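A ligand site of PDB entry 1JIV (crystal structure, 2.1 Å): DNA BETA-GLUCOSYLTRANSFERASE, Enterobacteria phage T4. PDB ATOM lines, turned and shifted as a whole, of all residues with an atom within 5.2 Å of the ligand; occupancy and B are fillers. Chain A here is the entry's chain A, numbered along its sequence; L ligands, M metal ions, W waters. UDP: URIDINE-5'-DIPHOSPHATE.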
ATOM      1  N   VAL A  18      -5.608   8.212  -9.537  1.00  0.00           N
ATOM      2  CA  VAL A  18      -4.488   8.810  -8.826  1.00  0.00           C
ATOM      3  C   VAL A  18      -4.737  10.201  -8.245  1.00  0.00           C
ATOM      4  O   VAL A  18      -4.501  10.429  -7.064  1.00  0.00           O
ATOM      5  CB  VAL A  18      -3.232   8.841  -9.720  1.00  0.00           C
ATOM      6  CG1 VAL A  18      -2.061   9.459  -8.974  1.00  0.00           C
ATOM      7  CG2 VAL A  18      -2.888   7.426 -10.151  1.00  0.00           C
ATOM      8  N   ASP A 100       4.011  18.932  -8.594  1.00  0.00           N
ATOM      9  CA  ASP A 100       4.539  18.574  -9.909  1.00  0.00           C
ATOM     10  C   ASP A 100       4.930  19.859 -10.649  1.00  0.00           C
ATOM     11  O   ASP A 100       4.076  20.689 -10.961  1.00  0.00           O
ATOM     12  CB  ASP A 100       3.496  17.790 -10.713  1.00  0.00           C
ATOM     13  CG  ASP A 100       4.052  17.243 -12.026  1.00  0.00           C
ATOM     14  OD1 ASP A 100       3.521  16.238 -12.518  1.00  0.00           O
ATOM     15  OD2 ASP A 100       5.009  17.833 -12.564  1.00  0.00           O
ATOM     16  N   LYS A 166       2.566  10.533   2.783  1.00  0.00           N
ATOM     17  CA  LYS A 166       2.297   9.106   2.868  1.00  0.00           C
ATOM     18  C   LYS A 166       2.940   8.462   4.100  1.00  0.00           C
ATOM     19  O   LYS A 166       2.345   7.574   4.715  1.00  0.00           O
ATOM     20  CB  LYS A 166       2.750   8.389   1.582  1.00  0.00           C
ATOM     21  CG  LYS A 166       1.671   7.428   1.047  1.00  0.00           C
ATOM     22  CD  LYS A 166       2.062   6.817  -0.301  1.00  0.00           C
ATOM     23  CE  LYS A 166       0.922   5.982  -0.890  1.00  0.00           C
ATOM     24  NZ  LYS A 166       1.156   5.603  -2.329  1.00  0.00           N
ATOM     25  N   TYR A 186       9.881  -0.024 -11.748  1.00  0.00           N
ATOM     26  CA  TYR A 186       9.641   1.420 -11.775  1.00  0.00           C
ATOM     27  C   TYR A 186       8.215   1.669 -12.230  1.00  0.00           C
ATOM     28  O   TYR A 186       7.772   1.107 -13.242  1.00  0.00           O
ATOM     29  CB  TYR A 186      10.626   2.120 -12.708  1.00  0.00           C
ATOM     30  CG  TYR A 186      10.385   3.625 -12.865  1.00  0.00           C
ATOM     31  CD1 TYR A 186       9.476   4.116 -13.807  1.00  0.00           C
ATOM     32  CD2 TYR A 186      11.094   4.548 -12.084  1.00  0.00           C
ATOM     33  CE1 TYR A 186       9.282   5.502 -13.969  1.00  0.00           C
ATOM     34  CE2 TYR A 186      10.898   5.920 -12.247  1.00  0.00           C
ATOM     35  CZ  TYR A 186       9.995   6.382 -13.190  1.00  0.00           C
ATOM     36  OH  TYR A 186       9.829   7.744 -13.359  1.00  0.00           O
ATOM     37  N   GLY A 187       7.482   2.508 -11.503  1.00  0.00           N
ATOM     38  CA  GLY A 187       6.112   2.786 -11.865  1.00  0.00           C
ATOM     39  C   GLY A 187       5.866   4.258 -12.125  1.00  0.00           C
ATOM     40  O   GLY A 187       6.227   5.102 -11.298  1.00  0.00           O
ATOM     41  N   GLY A 188       5.277   4.573 -13.263  1.00  0.00           N
ATOM     42  CA  GLY A 188       4.996   5.961 -13.583  1.00  0.00           C
ATOM     43  C   GLY A 188       4.510   6.175 -15.004  1.00  0.00           C
ATOM     44  O   GLY A 188       4.301   5.222 -15.753  1.00  0.00           O
ATOM     45  N   SER A 189       4.319   7.436 -15.374  1.00  0.00           N
ATOM     46  CA  SER A 189       3.881   7.754 -16.725  1.00  0.00           C
ATOM     47  C   SER A 189       5.109   8.117 -17.546  1.00  0.00           C
ATOM     48  O   SER A 189       6.242   8.081 -17.032  1.00  0.00           O
ATOM     49  CB  SER A 189       2.910   8.947 -16.714  1.00  0.00           C
ATOM     50  OG  SER A 189       3.605  10.151 -16.433  1.00  0.00           O
ATOM     51  N   ARG A 191       5.563  10.981 -18.693  1.00  0.00           N
ATOM     52  CA  ARG A 191       5.815  12.383 -18.390  1.00  0.00           C
ATOM     53  C   ARG A 191       6.251  13.178 -19.619  1.00  0.00           C
ATOM     54  O   ARG A 191       7.172  13.997 -19.551  1.00  0.00           O
ATOM     55  CB  ARG A 191       6.862  12.504 -17.274  1.00  0.00           C
ATOM     56  CG  ARG A 191       6.390  12.022 -15.903  1.00  0.00           C
ATOM     57  CD  ARG A 191       7.387  12.372 -14.810  1.00  0.00           C
ATOM     58  NE  ARG A 191       7.566  13.811 -14.668  1.00  0.00           N
ATOM     59  CZ  ARG A 191       6.676  14.634 -14.121  1.00  0.00           C
ATOM     60  NH1 ARG A 191       5.534  14.148 -13.643  1.00  0.00           N
ATOM     61  NH2 ARG A 191       6.916  15.930 -14.056  1.00  0.00           N
ATOM     62  N   ARG A 195      11.915  12.684 -19.167  1.00  0.00           N
ATOM     63  CA  ARG A 195      12.830  11.864 -18.393  1.00  0.00           C
ATOM     64  C   ARG A 195      13.242  10.647 -19.215  1.00  0.00           C
ATOM     65  O   ARG A 195      13.809   9.694 -18.677  1.00  0.00           O
ATOM     66  CB  ARG A 195      12.081  11.443 -17.123  1.00  0.00           C
ATOM     67  CG  ARG A 195      12.904  10.992 -15.951  1.00  0.00           C
ATOM     68  CD  ARG A 195      11.985  10.599 -14.782  1.00  0.00           C
ATOM     69  NE  ARG A 195      11.231  11.720 -14.228  1.00  0.00           N
ATOM     70  CZ  ARG A 195      10.362  11.623 -13.230  1.00  0.00           C
ATOM     71  NH1 ARG A 195      10.130  10.441 -12.659  1.00  0.00           N
ATOM     72  NH2 ARG A 195       9.733  12.703 -12.774  1.00  0.00           N
ATOM     73  N   PHE A 213       5.663  -0.311 -14.740  1.00  0.00           N
ATOM     74  CA  PHE A 213       4.210  -0.214 -14.647  1.00  0.00           C
ATOM     75  C   PHE A 213       3.718   1.235 -14.662  1.00  0.00           C
ATOM     76  O   PHE A 213       4.506   2.171 -14.535  1.00  0.00           O
ATOM     77  CB  PHE A 213       3.669  -0.955 -13.410  1.00  0.00           C
ATOM     78  CG  PHE A 213       4.114  -0.386 -12.076  1.00  0.00           C
ATOM     79  CD1 PHE A 213       5.363  -0.714 -11.551  1.00  0.00           C
ATOM     80  CD2 PHE A 213       3.254   0.416 -11.329  1.00  0.00           C
ATOM     81  CE1 PHE A 213       5.740  -0.260 -10.290  1.00  0.00           C
ATOM     82  CE2 PHE A 213       3.633   0.878 -10.073  1.00  0.00           C
ATOM     83  CZ  PHE A 213       4.880   0.535  -9.550  1.00  0.00           C
ATOM     84  N   GLY A 214       2.411   1.411 -14.848  1.00  0.00           N
ATOM     85  CA  GLY A 214       1.849   2.751 -14.914  1.00  0.00           C
ATOM     86  C   GLY A 214       1.307   3.026 -16.306  1.00  0.00           C
ATOM     87  O   GLY A 214       1.063   2.100 -17.078  1.00  0.00           O
ATOM     88  N   ASN A 215       1.127   4.305 -16.653  1.00  0.00           N
ATOM     89  CA  ASN A 215       0.591   4.688 -17.966  1.00  0.00           C
ATOM     90  C   ASN A 215       1.580   4.578 -19.118  1.00  0.00           C
ATOM     91  O   ASN A 215       1.176   4.568 -20.284  1.00  0.00           O
ATOM     92  CB  ASN A 215       0.072   6.134 -17.913  1.00  0.00           C
ATOM     93  CG  ASN A 215      -1.244   6.245 -17.178  1.00  0.00           C
ATOM     94  OD1 ASN A 215      -2.266   5.734 -17.624  1.00  0.00           O
ATOM     95  ND2 ASN A 215      -1.221   6.936 -16.047  1.00  0.00           N
ATOM     96  N   GLY A 236       1.071  -2.018 -17.365  1.00  0.00           N
ATOM     97  CA  GLY A 236      -0.168  -1.294 -17.124  1.00  0.00           C
ATOM     98  C   GLY A 236      -0.231  -0.635 -15.754  1.00  0.00           C
ATOM     99  O   GLY A 236       0.621  -0.834 -14.903  1.00  0.00           O
ATOM    100  N   LYS A 237      -1.290   0.129 -15.550  1.00  0.00           N
ATOM    101  CA  LYS A 237      -1.488   0.895 -14.335  1.00  0.00           C
ATOM    102  C   LYS A 237      -2.125   0.150 -13.172  1.00  0.00           C
ATOM    103  O   LYS A 237      -2.853  -0.831 -13.354  1.00  0.00           O
ATOM    104  CB  LYS A 237      -2.332   2.119 -14.680  1.00  0.00           C
ATOM    105  CG  LYS A 237      -2.365   3.210 -13.637  1.00  0.00           C
ATOM    106  CD  LYS A 237      -2.992   4.454 -14.237  1.00  0.00           C
ATOM    107  CE  LYS A 237      -3.003   5.604 -13.245  1.00  0.00           C
ATOM    108  NZ  LYS A 237      -3.485   6.836 -13.903  1.00  0.00           N
ATOM    109  N   ILE A 238      -1.813   0.609 -11.966  1.00  0.00           N
ATOM    110  CA  ILE A 238      -2.373   0.037 -10.753  1.00  0.00           C
ATOM    111  C   ILE A 238      -2.797   1.200  -9.872  1.00  0.00           C
ATOM    112  O   ILE A 238      -2.352   2.324 -10.070  1.00  0.00           O
ATOM    113  CB  ILE A 238      -1.339  -0.804  -9.976  1.00  0.00           C
ATOM    114  CG1 ILE A 238      -0.216   0.083  -9.470  1.00  0.00           C
ATOM    115  CG2 ILE A 238      -0.787  -1.916 -10.862  1.00  0.00           C
ATOM    116  CD1 ILE A 238       0.615  -0.546  -8.397  1.00  0.00           C
ATOM    117  N   PRO A 239      -3.673   0.947  -8.887  1.00  0.00           N
ATOM    118  CA  PRO A 239      -4.143   1.998  -7.976  1.00  0.00           C
ATOM    119  C   PRO A 239      -2.982   2.584  -7.176  1.00  0.00           C
ATOM    120  O   PRO A 239      -2.034   1.877  -6.838  1.00  0.00           O
ATOM    121  CB  PRO A 239      -5.129   1.266  -7.081  1.00  0.00           C
ATOM    122  CG  PRO A 239      -5.612   0.144  -7.934  1.00  0.00           C
ATOM    123  CD  PRO A 239      -4.364  -0.321  -8.617  1.00  0.00           C
ATOM    124  N   MET A 240      -3.069   3.866  -6.858  1.00  0.00           N
ATOM    125  CA  MET A 240      -2.027   4.518  -6.100  1.00  0.00           C
ATOM    126  C   MET A 240      -1.822   3.861  -4.734  1.00  0.00           C
ATOM    127  O   MET A 240      -0.684   3.756  -4.253  1.00  0.00           O
ATOM    128  CB  MET A 240      -2.353   5.995  -5.905  1.00  0.00           C
ATOM    129  CG  MET A 240      -1.201   6.770  -5.305  1.00  0.00           C
ATOM    130  SD  MET A 240      -1.659   8.404  -4.783  1.00  0.00           S
ATOM    131  CE  MET A 240      -0.659   8.563  -3.305  1.00  0.00           C
ATOM    132  N   VAL A 243       0.882   0.972  -4.798  1.00  0.00           N
ATOM    133  CA  VAL A 243       2.237   1.175  -5.327  1.00  0.00           C
ATOM    134  C   VAL A 243       3.386   0.555  -4.529  1.00  0.00           C
ATOM    135  O   VAL A 243       4.286  -0.051  -5.114  1.00  0.00           O
ATOM    136  CB  VAL A 243       2.496   2.672  -5.551  1.00  0.00           C
ATOM    137  CG1 VAL A 243       3.931   2.897  -6.034  1.00  0.00           C
ATOM    138  CG2 VAL A 243       1.520   3.208  -6.595  1.00  0.00           C
ATOM    139  N   ILE A 256      14.423   8.146 -10.114  1.00  0.00           N
ATOM    140  CA  ILE A 256      14.935   9.095 -11.082  1.00  0.00           C
ATOM    141  C   ILE A 256      13.933  10.239 -11.120  1.00  0.00           C
ATOM    142  O   ILE A 256      12.848  10.131 -10.543  1.00  0.00           O
ATOM    143  CB  ILE A 256      15.080   8.496 -12.503  1.00  0.00           C
ATOM    144  CG1 ILE A 256      13.773   7.822 -12.925  1.00  0.00           C
ATOM    145  CG2 ILE A 256      16.252   7.527 -12.548  1.00  0.00           C
ATOM    146  CD1 ILE A 256      13.778   7.311 -14.353  1.00  0.00           C
ATOM    147  N   ASP A 258      12.766  14.400 -13.110  1.00  0.00           N
ATOM    148  CA  ASP A 258      12.907  15.410 -14.137  1.00  0.00           C
ATOM    149  C   ASP A 258      14.172  16.216 -13.866  1.00  0.00           C
ATOM    150  O   ASP A 258      14.626  16.287 -12.726  1.00  0.00           O
ATOM    151  CB  ASP A 258      11.705  16.351 -14.132  1.00  0.00           C
ATOM    152  CG  ASP A 258      10.447  15.714 -14.717  1.00  0.00           C
ATOM    153  OD1 ASP A 258      10.384  14.463 -14.784  1.00  0.00           O
ATOM    154  OD2 ASP A 258       9.528  16.471 -15.084  1.00  0.00           O
ATOM    155  N   TYR A 261      14.143  18.328 -11.028  1.00  0.00           N
ATOM    156  CA  TYR A 261      13.895  17.603  -9.782  1.00  0.00           C
ATOM    157  C   TYR A 261      15.196  17.259  -9.061  1.00  0.00           C
ATOM    158  O   TYR A 261      15.225  17.148  -7.827  1.00  0.00           O
ATOM    159  CB  TYR A 261      13.127  16.306 -10.049  1.00  0.00           C
ATOM    160  CG  TYR A 261      11.638  16.487 -10.224  1.00  0.00           C
ATOM    161  CD1 TYR A 261      11.087  17.751 -10.409  1.00  0.00           C
ATOM    162  CD2 TYR A 261      10.778  15.390 -10.214  1.00  0.00           C
ATOM    163  CE1 TYR A 261       9.728  17.925 -10.578  1.00  0.00           C
ATOM    164  CE2 TYR A 261       9.407  15.544 -10.393  1.00  0.00           C
ATOM    165  CZ  TYR A 261       8.887  16.818 -10.574  1.00  0.00           C
ATOM    166  OH  TYR A 261       7.539  16.998 -10.749  1.00  0.00           O
ATOM    167  N   THR A 267      10.462  13.458  -4.237  1.00  0.00           N
ATOM    168  CA  THR A 267       9.141  13.013  -4.642  1.00  0.00           C
ATOM    169  C   THR A 267       8.501  11.874  -3.866  1.00  0.00           C
ATOM    170  O   THR A 267       9.157  11.156  -3.109  1.00  0.00           O
ATOM    171  CB  THR A 267       9.150  12.657  -6.136  1.00  0.00           C
ATOM    172  OG1 THR A 267      10.063  11.583  -6.365  1.00  0.00           O
ATOM    173  CG2 THR A 267       9.601  13.866  -6.969  1.00  0.00           C
ATOM    174  N   LEU A 268       7.198  11.724  -4.076  1.00  0.00           N
ATOM    175  CA  LEU A 268       6.420  10.689  -3.426  1.00  0.00           C
ATOM    176  C   LEU A 268       7.023   9.300  -3.659  1.00  0.00           C
ATOM    177  O   LEU A 268       7.067   8.480  -2.756  1.00  0.00           O
ATOM    178  CB  LEU A 268       4.975  10.732  -3.942  1.00  0.00           C
ATOM    179  CG  LEU A 268       3.946   9.804  -3.287  1.00  0.00           C
ATOM    180  CD1 LEU A 268       3.867  10.075  -1.799  1.00  0.00           C
ATOM    181  CD2 LEU A 268       2.583  10.006  -3.939  1.00  0.00           C
ATOM    182  N   ARG A 269       7.503   9.032  -4.880  1.00  0.00           N
ATOM    183  CA  ARG A 269       8.079   7.720  -5.152  1.00  0.00           C
ATOM    184  C   ARG A 269       9.264   7.407  -4.234  1.00  0.00           C
ATOM    185  O   ARG A 269       9.512   6.232  -3.936  1.00  0.00           O
ATOM    186  CB  ARG A 269       8.516   7.579  -6.624  1.00  0.00           C
ATOM    187  CG  ARG A 269       9.754   8.340  -7.021  1.00  0.00           C
ATOM    188  CD  ARG A 269      10.243   7.929  -8.423  1.00  0.00           C
ATOM    189  NE  ARG A 269       9.216   8.140  -9.441  1.00  0.00           N
ATOM    190  CZ  ARG A 269       8.505   7.178 -10.019  1.00  0.00           C
ATOM    191  NH1 ARG A 269       8.697   5.899  -9.685  1.00  0.00           N
ATOM    192  NH2 ARG A 269       7.580   7.488 -10.912  1.00  0.00           N
ATOM    193  N   GLU A 272       7.483   5.896  -1.346  1.00  0.00           N
ATOM    194  CA  GLU A 272       6.780   4.656  -1.702  1.00  0.00           C
ATOM    195  C   GLU A 272       7.810   3.559  -1.914  1.00  0.00           C
ATOM    196  O   GLU A 272       7.547   2.389  -1.666  1.00  0.00           O
ATOM    197  CB  GLU A 272       5.974   4.823  -2.986  1.00  0.00           C
ATOM    198  CG  GLU A 272       4.917   5.922  -2.934  1.00  0.00           C
ATOM    199  CD  GLU A 272       4.348   6.234  -4.305  1.00  0.00           C
ATOM    200  OE1 GLU A 272       5.150   6.314  -5.261  1.00  0.00           O
ATOM    201  OE2 GLU A 272       3.115   6.397  -4.428  1.00  0.00           O
HETATM  202  N1  UDP L   1       1.451   5.706  -9.745  1.00  0.00           N
HETATM  203  C2  UDP L   1       0.275   5.023  -9.492  1.00  0.00           C
HETATM  204  N3  UDP L   1       0.079   3.906 -10.274  1.00  0.00           N
HETATM  205  C4  UDP L   1       0.918   3.421 -11.262  1.00  0.00           C
HETATM  206  C5  UDP L   1       2.117   4.182 -11.450  1.00  0.00           C
HETATM  207  C6  UDP L   1       2.334   5.277 -10.704  1.00  0.00           C
HETATM  208  O2  UDP L   1      -0.519   5.358  -8.639  1.00  0.00           O
HETATM  209  O4  UDP L   1       0.591   2.413 -11.899  1.00  0.00           O
HETATM  210  C1' UDP L   1       1.690   6.939  -8.957  1.00  0.00           C
HETATM  211  C2' UDP L   1       2.612   6.745  -7.756  1.00  0.00           C
HETATM  212  O2' UDP L   1       2.163   7.521  -6.665  1.00  0.00           O
HETATM  213  C3' UDP L   1       3.960   7.214  -8.301  1.00  0.00           C
HETATM  214  C4' UDP L   1       3.550   8.335  -9.246  1.00  0.00           C
HETATM  215  O4' UDP L   1       2.285   7.904  -9.808  1.00  0.00           O
HETATM  216  O3' UDP L   1       4.799   7.716  -7.283  1.00  0.00           O
HETATM  217  C5' UDP L   1       4.529   8.588 -10.363  1.00  0.00           C
HETATM  218  O5' UDP L   1       4.268   9.842 -10.977  1.00  0.00           O
HETATM  219  PA  UDP L   1       5.145  10.352 -12.205  1.00  0.00           P
HETATM  220  O1A UDP L   1       5.159   9.283 -13.227  1.00  0.00           O
HETATM  221  O2A UDP L   1       4.673  11.714 -12.567  1.00  0.00           O
HETATM  222  O3A UDP L   1       6.615  10.432 -11.571  1.00  0.00           O
HETATM  223  PB  UDP L   1       7.217  11.387 -10.449  1.00  0.00           P
HETATM  224  O1B UDP L   1       7.415  12.653 -11.209  1.00  0.00           O
HETATM  225  O2B UDP L   1       8.450  10.640 -10.093  1.00  0.00           O
HETATM  226  O3B UDP L   1       6.137  11.404  -9.427  1.00  0.00           O
HETATM  227 MG    MG M   1       3.824  13.654  -7.214  1.00  0.00          MG
HETATM  228  O   HOH W   1       5.859  13.960  -7.512  1.00  0.00           O
HETATM  229  O   HOH W   2       6.081  10.270  -7.011  1.00  0.00           O
HETATM  230  O   HOH W   3       7.493   8.586 -14.606  1.00  0.00           O
HETATM  231  O   HOH W   4      10.965  11.496  -9.133  1.00  0.00           O
HETATM  232  O   HOH W   5       1.184   8.937 -12.530  1.00  0.00           O
HETATM  233  O   HOH W   6       2.680  11.622 -14.273  1.00  0.00           O
HETATM  234  O   HOH W   7       1.225  10.065  -7.366  1.00  0.00           O
HETATM  235  O   HOH W   8       4.259  13.048  -9.406  1.00  0.00           O
HETATM  236  O   HOH W   9       6.011  14.814 -10.361  1.00  0.00           O
HETATM  237  O   HOH W  10       1.092  11.077  -9.860  1.00  0.00           O
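NH2 of Arg 195 is in salt-bridge range of O1B of the ligand.
An oxygen (O1A) of the ligand is in hydrogen-bond range of the backbone NH (N) of Ser 189 (3.0 Å).
NE of Arg 269 is in salt-bridge range of O2B of the ligand, at 2.7 Å.
O of Ile 238 sits at hydrogen-bond distance from N3 of the ligand (2.9 Å).
N of Met 240 sits close to O2 of the ligand (3.4 Å).
An oxygen (O2A) of the ligand is in salt-bridge range of the guanidinium group of Arg 191.
The backbone NH (N) of Ile 238 sits at hydrogen-bond distance from an oxygen (O4) of the ligand (3.0 Å).
OE1 of Glu 272 lies within hydrogen-bond range of O3' of the ligand (2.5 Å).
The backbone carbonyl oxygen (O) of Met 240 sits at hydrogen-bond distance from the side-chain amino group (NZ) of Lys 166 (3.2 Å).
The side-chain amino group (NZ) of Lys 166 lies within salt-bridge range of the side-chain carboxylate (OE2) of Glu 272 (3.0 Å).
The backbone NH (N) of Arg 191 lies within hydrogen-bond range of the side-chain hydroxyl (OG) of Ser 189, at 3.1 Å.
The side-chain carboxylate (OD1) of Asp 258 lies within salt-bridge range of the guanidinium group (NH2) of Arg 195.
O of Gly 214 is in hydrogen-bond range of N of Lys 237, at 3.4 Å.
The guanidinium group of Arg 269 sits at hydrogen-bond distance from the side-chain hydroxyl of Tyr 186, 3.3 Å away.
N of Gly 188 lies within hydrogen-bond range of O of Phe 213 (2.8 Å).
N of Gly 214 lies within hydrogen-bond range of O of Gly 236 (2.9 Å).
Val 18 touches the ligand.
C of Gly 187 touches C5 of the ligand (3.8 Å).
Gly 188 touches the ligand (CA to O1A, 3.3 Å).
CD2 of Phe 213 touches O4 of the ligand (3.4 Å).
CA of Gly 214 touches O4 of the ligand (3.3 Å).
CG of Lys 237 touches O4 of the ligand, at 3.5 Å.
Pro 239 touches the ligand.
CG2 of Val 243 touches O2 of the ligand, at 3.6 Å.
Tyr 261 touches the ligand (CE2 to O1B, 3.6 Å).
CD2 of Leu 268 touches O2' of the ligand, 3.7 Å away.
Hydrophobic or aromatic side chains within 4 Å of the ligand: Val 18, Phe 213, Ile 238, Met 240, Val 243, Tyr 261 and Leu 268.
Within 4 Å of the ligand: Val 18, Gly 187, Gly 188, Ser 189, Arg 191, Arg 195, Phe 213, Gly 214, Lys 237, Ile 238, Pro 239, Met 240, Val 243, Tyr 261, Leu 268, Arg 269 and Glu 272.
The nearest printed residue that does not touch the ligand is Thr 267 (4.2 Å).
Water W6 lies within hydrogen-bond range of O2A of the ligand (2.6 Å) and OG of Ser 189 (2.8 Å).
Water W2 lies within hydrogen-bond range of O3B of the ligand (2.7 Å), N of Arg 269 (2.8 Å) and N of Leu 268 (3.5 Å).
Water W9 lies within hydrogen-bond range of the side-chain hydroxyl (OH) of Tyr 261, an oxygen (O1B) of the ligand and the guanidinium group (NH1) of Arg 191.
Water W3 lies within hydrogen-bond range of O of Ser 189 (2.8 Å), OH of Tyr 186 (2.8 Å) and O1A of the ligand (2.8 Å).
Water W4 lies within hydrogen-bond range of O of Ile 256 (2.7 Å), O2B of the ligand (2.8 Å) and OG1 of Thr 267 (2.9 Å).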
